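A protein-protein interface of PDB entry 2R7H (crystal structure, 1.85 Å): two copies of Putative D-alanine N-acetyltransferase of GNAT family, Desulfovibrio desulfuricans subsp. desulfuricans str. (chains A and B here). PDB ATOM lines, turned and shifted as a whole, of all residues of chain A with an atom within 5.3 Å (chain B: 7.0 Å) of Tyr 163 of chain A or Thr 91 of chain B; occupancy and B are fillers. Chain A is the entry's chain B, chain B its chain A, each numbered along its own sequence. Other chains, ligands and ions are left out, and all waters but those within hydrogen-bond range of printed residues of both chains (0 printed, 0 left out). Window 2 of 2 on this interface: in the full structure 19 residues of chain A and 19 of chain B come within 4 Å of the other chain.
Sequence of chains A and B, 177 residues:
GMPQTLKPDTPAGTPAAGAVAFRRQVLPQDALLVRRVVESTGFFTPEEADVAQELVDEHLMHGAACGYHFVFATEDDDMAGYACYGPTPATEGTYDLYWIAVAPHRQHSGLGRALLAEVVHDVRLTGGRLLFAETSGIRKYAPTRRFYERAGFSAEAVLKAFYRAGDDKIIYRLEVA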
ATOM      1  N   GLU A 134     -16.668 -16.878  33.667  1.00  0.00           N
ATOM      2  CA  GLU A 134     -15.373 -16.394  33.171  1.00  0.00           C
ATOM      3  C   GLU A 134     -14.826 -15.362  34.126  1.00  0.00           C
ATOM      4  O   GLU A 134     -15.582 -14.548  34.635  1.00  0.00           O
ATOM      5  CB  GLU A 134     -15.554 -15.714  31.813  1.00  0.00           C
ATOM      6  CG  GLU A 134     -16.170 -16.580  30.802  1.00  0.00           C
ATOM      7  CD  GLU A 134     -16.244 -15.929  29.437  1.00  0.00           C
ATOM      8  OE1 GLU A 134     -16.325 -14.690  29.353  1.00  0.00           O
ATOM      9  OE2 GLU A 134     -16.244 -16.678  28.461  1.00  0.00           O
ATOM     10  N   THR A 135     -13.526 -15.409  34.399  1.00  0.00           N
ATOM     11  CA  THR A 135     -12.938 -14.396  35.234  1.00  0.00           C
ATOM     12  C   THR A 135     -11.511 -14.116  34.772  1.00  0.00           C
ATOM     13  O   THR A 135     -11.014 -14.734  33.806  1.00  0.00           O
ATOM     14  CB  THR A 135     -13.049 -14.733  36.749  1.00  0.00           C
ATOM     15  OG1 THR A 135     -12.734 -13.561  37.497  1.00  0.00           O
ATOM     16  CG2 THR A 135     -12.140 -15.889  37.147  1.00  0.00           C
ATOM     17  N   SER A 136     -10.884 -13.166  35.443  1.00  0.00           N
ATOM     18  CA  SER A 136      -9.523 -12.748  35.141  1.00  0.00           C
ATOM     19  C   SER A 136      -8.500 -13.551  35.930  1.00  0.00           C
ATOM     20  O   SER A 136      -8.772 -14.060  37.004  1.00  0.00           O
ATOM     21  CB  SER A 136      -9.367 -11.254  35.407  1.00  0.00           C
ATOM     22  OG  SER A 136      -8.019 -10.882  35.414  1.00  0.00           O
ATOM     23  N   ALA A 161      -3.564 -13.468  27.971  1.00  0.00           N
ATOM     24  CA  ALA A 161      -3.659 -12.033  27.696  1.00  0.00           C
ATOM     25  C   ALA A 161      -4.936 -11.633  26.994  1.00  0.00           C
ATOM     26  O   ALA A 161      -4.931 -10.715  26.225  1.00  0.00           O
ATOM     27  CB  ALA A 161      -2.424 -11.554  26.882  1.00  0.00           C
ATOM     28  N   PHE A 162      -6.050 -12.291  27.306  1.00  0.00           N
ATOM     29  CA  PHE A 162      -7.317 -12.014  26.681  1.00  0.00           C
ATOM     30  C   PHE A 162      -7.811 -10.598  26.918  1.00  0.00           C
ATOM     31  O   PHE A 162      -8.177  -9.894  25.949  1.00  0.00           O
ATOM     32  CB  PHE A 162      -8.345 -13.041  27.188  1.00  0.00           C
ATOM     33  CG  PHE A 162      -9.687 -12.919  26.555  1.00  0.00           C
ATOM     34  CD1 PHE A 162      -9.964 -13.629  25.412  1.00  0.00           C
ATOM     35  CD2 PHE A 162     -10.681 -12.145  27.123  1.00  0.00           C
ATOM     36  CE1 PHE A 162     -11.187 -13.527  24.802  1.00  0.00           C
ATOM     37  CE2 PHE A 162     -11.923 -12.058  26.525  1.00  0.00           C
ATOM     38  CZ  PHE A 162     -12.170 -12.754  25.358  1.00  0.00           C
ATOM     39  N   TYR A 163      -7.779 -10.152  28.158  1.00  0.00           N
ATOM     40  CA  TYR A 163      -8.281  -8.785  28.465  1.00  0.00           C
ATOM     41  C   TYR A 163      -7.276  -7.688  28.155  1.00  0.00           C
ATOM     42  O   TYR A 163      -7.671  -6.622  27.711  1.00  0.00           O
ATOM     43  CB  TYR A 163      -8.761  -8.673  29.895  1.00  0.00           C
ATOM     44  CG  TYR A 163      -9.841  -9.637  30.277  1.00  0.00           C
ATOM     45  CD1 TYR A 163     -11.157  -9.437  29.875  1.00  0.00           C
ATOM     46  CD2 TYR A 163      -9.570 -10.719  31.095  1.00  0.00           C
ATOM     47  CE1 TYR A 163     -12.164 -10.292  30.248  1.00  0.00           C
ATOM     48  CE2 TYR A 163     -10.592 -11.590  31.504  1.00  0.00           C
ATOM     49  CZ  TYR A 163     -11.888 -11.371  31.075  1.00  0.00           C
ATOM     50  OH  TYR A 163     -12.890 -12.246  31.436  1.00  0.00           O
ATOM     51  N   ARG A 164      -5.996  -7.957  28.395  1.00  0.00           N
ATOM     52  CA  ARG A 164      -4.875  -7.051  28.126  1.00  0.00           C
ATOM     53  C   ARG A 164      -3.619  -7.835  28.434  1.00  0.00           C
ATOM     54  O   ARG A 164      -3.703  -8.946  28.966  1.00  0.00           O
ATOM     55  CB  ARG A 164      -4.920  -5.753  28.953  1.00  0.00           C
ATOM     56  CG  ARG A 164      -4.928  -5.926  30.469  1.00  0.00           C
ATOM     57  CD  ARG A 164      -5.112  -4.609  31.276  1.00  0.00           C
ATOM     58  NE  ARG A 164      -6.341  -3.924  30.871  1.00  0.00           N
ATOM     59  CZ  ARG A 164      -7.591  -4.308  31.177  1.00  0.00           C
ATOM     60  NH1 ARG A 164      -7.842  -5.386  31.929  1.00  0.00           N
ATOM     61  NH2 ARG A 164      -8.623  -3.599  30.707  1.00  0.00           N
ATOM     62  N   ALA A 165      -2.454  -7.256  28.124  1.00  0.00           N
ATOM     63  CA  ALA A 165      -1.180  -7.907  28.393  1.00  0.00           C
ATOM     64  C   ALA A 165      -1.122  -8.310  29.879  1.00  0.00           C
ATOM     65  O   ALA A 165      -1.470  -7.527  30.742  1.00  0.00           O
ATOM     66  CB  ALA A 165      -0.002  -6.961  28.014  1.00  0.00           C
ATOM     67  N   ASP A 167      -3.195 -10.161  31.514  1.00  0.00           N
ATOM     68  CA  ASP A 167      -4.526 -10.376  32.091  1.00  0.00           C
ATOM     69  C   ASP A 167      -5.273 -11.473  31.277  1.00  0.00           C
ATOM     70  O   ASP A 167      -5.916 -11.213  30.287  1.00  0.00           O
ATOM     71  CB  ASP A 167      -5.284  -9.058  32.120  1.00  0.00           C
ATOM     72  CG  ASP A 167      -6.531  -9.120  32.962  1.00  0.00           C
ATOM     73  OD1 ASP A 167      -7.019 -10.218  33.266  1.00  0.00           O
ATOM     74  OD2 ASP A 167      -7.032  -8.052  33.352  1.00  0.00           O
ATOM     75  N   ASP A 168      -5.159 -12.703  31.759  1.00  0.00           N
ATOM     76  CA  ASP A 168      -5.746 -13.879  31.130  1.00  0.00           C
ATOM     77  C   ASP A 168      -7.193 -14.079  31.498  1.00  0.00           C
ATOM     78  O   ASP A 168      -7.599 -13.656  32.576  1.00  0.00           O
ATOM     79  CB  ASP A 168      -5.020 -15.127  31.614  1.00  0.00           C
ATOM     80  CG  ASP A 168      -3.531 -15.107  31.323  1.00  0.00           C
ATOM     81  OD1 ASP A 168      -3.064 -14.275  30.513  1.00  0.00           O
ATOM     82  OD2 ASP A 168      -2.842 -15.946  31.925  1.00  0.00           O
ATOM     83  N   LYS A 169      -7.964 -14.712  30.601  1.00  0.00           N
ATOM     84  CA  LYS A 169      -9.354 -15.036  30.890  1.00  0.00           C
ATOM     85  C   LYS A 169      -9.320 -16.485  31.253  1.00  0.00           C
ATOM     86  O   LYS A 169      -8.736 -17.259  30.493  1.00  0.00           O
ATOM     87  CB  LYS A 169     -10.294 -14.860  29.683  1.00  0.00           C
ATOM     88  CG  LYS A 169     -11.790 -15.163  30.072  1.00  0.00           C
ATOM     89  CD  LYS A 169     -12.783 -14.679  29.068  1.00  0.00           C
ATOM     90  CE  LYS A 169     -12.803 -15.427  27.828  1.00  0.00           C
ATOM     91  NZ  LYS A 169     -14.010 -15.010  27.013  1.00  0.00           N
ATOM     92  N   PRO B  87     -14.787  -6.003  17.909  1.00  0.00           N
ATOM     93  CA  PRO B  87     -13.979  -5.940  19.129  1.00  0.00           C
ATOM     94  C   PRO B  87     -14.639  -6.730  20.262  1.00  0.00           C
ATOM     95  O   PRO B  87     -15.865  -6.742  20.376  1.00  0.00           O
ATOM     96  CB  PRO B  87     -13.935  -4.440  19.449  1.00  0.00           C
ATOM     97  CG  PRO B  87     -15.208  -3.935  18.887  1.00  0.00           C
ATOM     98  CD  PRO B  87     -15.411  -4.701  17.604  1.00  0.00           C
ATOM     99  N   THR B  88     -13.841  -7.457  21.037  1.00  0.00           N
ATOM    100  CA  THR B  88     -14.382  -8.250  22.136  1.00  0.00           C
ATOM    101  C   THR B  88     -14.737  -7.310  23.310  1.00  0.00           C
ATOM    102  O   THR B  88     -13.877  -6.576  23.773  1.00  0.00           O
ATOM    103  CB  THR B  88     -13.409  -9.327  22.550  1.00  0.00           C
ATOM    104  OG1 THR B  88     -13.135 -10.121  21.384  1.00  0.00           O
ATOM    105  CG2 THR B  88     -14.003 -10.215  23.637  1.00  0.00           C
ATOM    106  N   PRO B  89     -15.989  -7.355  23.816  1.00  0.00           N
ATOM    107  CA  PRO B  89     -16.291  -6.413  24.905  1.00  0.00           C
ATOM    108  C   PRO B  89     -15.457  -6.653  26.152  1.00  0.00           C
ATOM    109  O   PRO B  89     -15.097  -7.764  26.443  1.00  0.00           O
ATOM    110  CB  PRO B  89     -17.782  -6.663  25.194  1.00  0.00           C
ATOM    111  CG  PRO B  89     -18.300  -7.434  24.055  1.00  0.00           C
ATOM    112  CD  PRO B  89     -17.137  -8.239  23.538  1.00  0.00           C
ATOM    113  N   ALA B  90     -15.125  -5.581  26.848  1.00  0.00           N
ATOM    114  CA  ALA B  90     -14.346  -5.619  28.093  1.00  0.00           C
ATOM    115  C   ALA B  90     -12.886  -6.035  27.925  1.00  0.00           C
ATOM    116  O   ALA B  90     -12.322  -6.537  28.860  1.00  0.00           O
ATOM    117  CB  ALA B  90     -15.037  -6.541  29.147  1.00  0.00           C
ATOM    118  N   THR B  91     -12.281  -5.843  26.753  1.00  0.00           N
ATOM    119  CA  THR B  91     -10.882  -6.213  26.541  1.00  0.00           C
ATOM    120  C   THR B  91     -10.181  -5.040  25.884  1.00  0.00           C
ATOM    121  O   THR B  91     -10.825  -4.135  25.381  1.00  0.00           O
ATOM    122  CB  THR B  91     -10.728  -7.397  25.543  1.00  0.00           C
ATOM    123  OG1 THR B  91     -11.203  -6.984  24.253  1.00  0.00           O
ATOM    124  CG2 THR B  91     -11.458  -8.633  25.971  1.00  0.00           C
ATOM    125  N   GLU B  92      -8.855  -5.061  25.923  1.00  0.00           N
ATOM    126  CA  GLU B  92      -8.049  -4.084  25.239  1.00  0.00           C
ATOM    127  C   GLU B  92      -7.419  -4.787  24.043  1.00  0.00           C
ATOM    128  O   GLU B  92      -6.598  -5.648  24.211  1.00  0.00           O
ATOM    129  CB  GLU B  92      -6.970  -3.512  26.147  1.00  0.00           C
ATOM    130  CG  GLU B  92      -7.530  -2.627  27.251  1.00  0.00           C
ATOM    131  CD  GLU B  92      -6.447  -2.043  28.169  1.00  0.00           C
ATOM    132  OE1 GLU B  92      -5.237  -2.390  28.021  1.00  0.00           O
ATOM    133  OE2 GLU B  92      -6.829  -1.237  29.053  1.00  0.00           O
ATOM    134  N   GLY B  93      -7.857  -4.465  22.843  1.00  0.00           N
ATOM    135  CA  GLY B  93      -7.264  -5.025  21.633  1.00  0.00           C
ATOM    136  C   GLY B  93      -7.520  -6.472  21.269  1.00  0.00           C
ATOM    137  O   GLY B  93      -6.703  -7.060  20.580  1.00  0.00           O
ATOM    138  N   THR B  94      -8.629  -7.038  21.744  1.00  0.00           N
ATOM    139  CA  THR B  94      -9.025  -8.410  21.440  1.00  0.00           C
ATOM    140  C   THR B  94     -10.239  -8.300  20.571  1.00  0.00           C
ATOM    141  O   THR B  94     -11.089  -7.427  20.792  1.00  0.00           O
ATOM    142  CB  THR B  94      -9.284  -9.249  22.678  1.00  0.00           C
ATOM    143  OG1 THR B  94      -8.039  -9.415  23.365  1.00  0.00           O
ATOM    144  CG2 THR B  94      -9.813 -10.653  22.329  1.00  0.00           C
ATOM    145  N   TYR B  95     -10.259  -9.142  19.531  1.00  0.00           N
ATOM    146  CA  TYR B  95     -11.295  -9.225  18.516  1.00  0.00           C
ATOM    147  C   TYR B  95     -11.736 -10.650  18.292  1.00  0.00           C
ATOM    148  O   TYR B  95     -11.004 -11.610  18.569  1.00  0.00           O
ATOM    149  CB  TYR B  95     -10.787  -8.629  17.179  1.00  0.00           C
ATOM    150  CG  TYR B  95     -10.586  -7.136  17.244  1.00  0.00           C
ATOM    151  CD1 TYR B  95      -9.467  -6.605  17.866  1.00  0.00           C
ATOM    152  CD2 TYR B  95     -11.498  -6.256  16.673  1.00  0.00           C
ATOM    153  CE1 TYR B  95      -9.283  -5.227  17.986  1.00  0.00           C
ATOM    154  CE2 TYR B  95     -11.318  -4.893  16.773  1.00  0.00           C
ATOM    155  CZ  TYR B  95     -10.199  -4.387  17.415  1.00  0.00           C
ATOM    156  OH  TYR B  95      -9.984  -3.019  17.528  1.00  0.00           O
ATOM    157  N   ARG B 129      -4.421  -6.750  19.173  1.00  0.00           N
ATOM    158  CA  ARG B 129      -3.446  -7.740  19.593  1.00  0.00           C
ATOM    159  C   ARG B 129      -3.795  -9.178  19.260  1.00  0.00           C
ATOM    160  O   ARG B 129      -2.906  -9.998  18.916  1.00  0.00           O
ATOM    161  CB  ARG B 129      -3.319  -7.686  21.141  1.00  0.00           C
ATOM    162  CG  ARG B 129      -2.988  -6.300  21.694  1.00  0.00           C
ATOM    163  CD  ARG B 129      -2.886  -6.225  23.217  1.00  0.00           C
ATOM    164  NE  ARG B 129      -4.100  -6.680  23.897  1.00  0.00           N
ATOM    165  CZ  ARG B 129      -4.314  -7.889  24.452  1.00  0.00           C
ATOM    166  NH1 ARG B 129      -3.349  -8.787  24.576  1.00  0.00           N
ATOM    167  NH2 ARG B 129      -5.507  -8.166  24.982  1.00  0.00           N
ATOM    168  N   LEU B 130      -5.072  -9.514  19.463  1.00  0.00           N
ATOM    169  CA  LEU B 130      -5.545 -10.857  19.292  1.00  0.00           C
ATOM    170  C   LEU B 130      -6.828 -10.952  18.535  1.00  0.00           C
ATOM    171  O   LEU B 130      -7.647 -10.070  18.650  1.00  0.00           O
ATOM    172  CB  LEU B 130      -5.800 -11.431  20.674  1.00  0.00           C
ATOM    173  CG  LEU B 130      -4.583 -11.744  21.541  1.00  0.00           C
ATOM    174  CD1 LEU B 130      -5.023 -11.875  23.037  1.00  0.00           C
ATOM    175  CD2 LEU B 130      -3.865 -12.953  21.010  1.00  0.00           C
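O of Tyr 163 of chain A lies within hydrogen-bond range of N of Glu 92 of chain B, at 2.7 Å.
The guanidinium group (NE) of Arg 164 of chain A lies within salt-bridge range of the side-chain carboxylate (OE2) of Glu 92 of chain B.
OG1 of Thr 94 of chain B sits at hydrogen-bond distance from O of Phe 162 of chain A, at 2.6 Å.
The guanidinium group of Arg 129 of chain B lies within hydrogen-bond range of the backbone carbonyl oxygen of Ala 161 of chain A, 2.9 Å away.
O of Phe 162 of chain A sits at hydrogen-bond distance from NH2 of Arg 129 of chain B, at 3.3 Å.
N of Arg 164 of chain A sits close to NH2 of Arg 129 of chain B (3.5 Å).
Ser 136 of chain A touches none of the printed residues of chain B.
Of chain B, only Ala 90 (3.3 Å), Thr 91 (3.4 Å), Glu 92 (2.7 Å) and Arg 129 (3.7 Å) come within 4 Å of Tyr 163 of chain A.
Of the printed residues of chain B, Arg 164 of chain A touches Glu 92 and Arg 129.
Of the printed residues of chain A, Glu 92 of chain B touches Tyr 163 (2.7 Å) and Arg 164 (3.3 Å).
The nearest residue of chain B that does not touch Tyr 163 of chain A is Thr 94 of chain B (4.9 Å).
The nearest printed residue of chain A that does not touch Thr 91 of chain B is Arg 164 of chain A (5.3 Å).
The nearest printed residue of chain A that does not touch Arg 129 of chain B is Asp 167 of chain A (6.1 Å).
Among the printed residues, pairs that only touch across the chains: Ala 161 of chain A with Leu 130 of chain B, Phe 162 of chain A with Thr 88 of chain B, Phe 162 of chain A with Thr 91 of chain B, Tyr 163 of chain A with Ala 90 of chain B, Tyr 163 of chain A with Thr 91 of chain B, Tyr 163 of chain A with Arg 129 of chain B and Ala 165 of chain A with Arg 129 of chain B.
No position is printed for both chains.
Of the 13 pairs that touch across the chains among the printed residues, none has its exchanged pair printed and touching as well.
The backbone carbonyl oxygen of Thr 88 of chain B is in hydrogen-bond range of the side-chain hydroxyl of Thr 91 of chain B, at 2.7 Å.
O of Gly 93 of chain B lies within hydrogen-bond range of N of Arg 129 of chain B (2.7 Å).
The backbone NH (N) of Tyr 95 of chain B lies within hydrogen-bond range of the backbone carbonyl oxygen (O) of Leu 130 of chain B (2.9 Å).
The side-chain carboxylate (OD1) of Asp 168 of chain A lies within hydrogen-bond range of the backbone NH (N) of Ala 161 of chain A, 2.7 Å away.
N of Phe 162 of chain A is in hydrogen-bond range of O of Asp 167 of chain A (3.2 Å).
The guanidinium group (NH1) of Arg 164 of chain A lies within salt-bridge range of the side-chain carboxylate (OD2) of Asp 167 of chain A (3.1 Å).
Hydrophobic or aromatic side chains of chain B that line the printed part of chain A: Leu 130.
Among the printed residues, 13 pairs touch across the chains.
Among the printed residues, Asp or Glu carboxylates within 4 Å of a Lys or Arg side-chain nitrogen of the other chain: Arg 164 of chain A with Glu 92 of chain B (3.3 Å).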
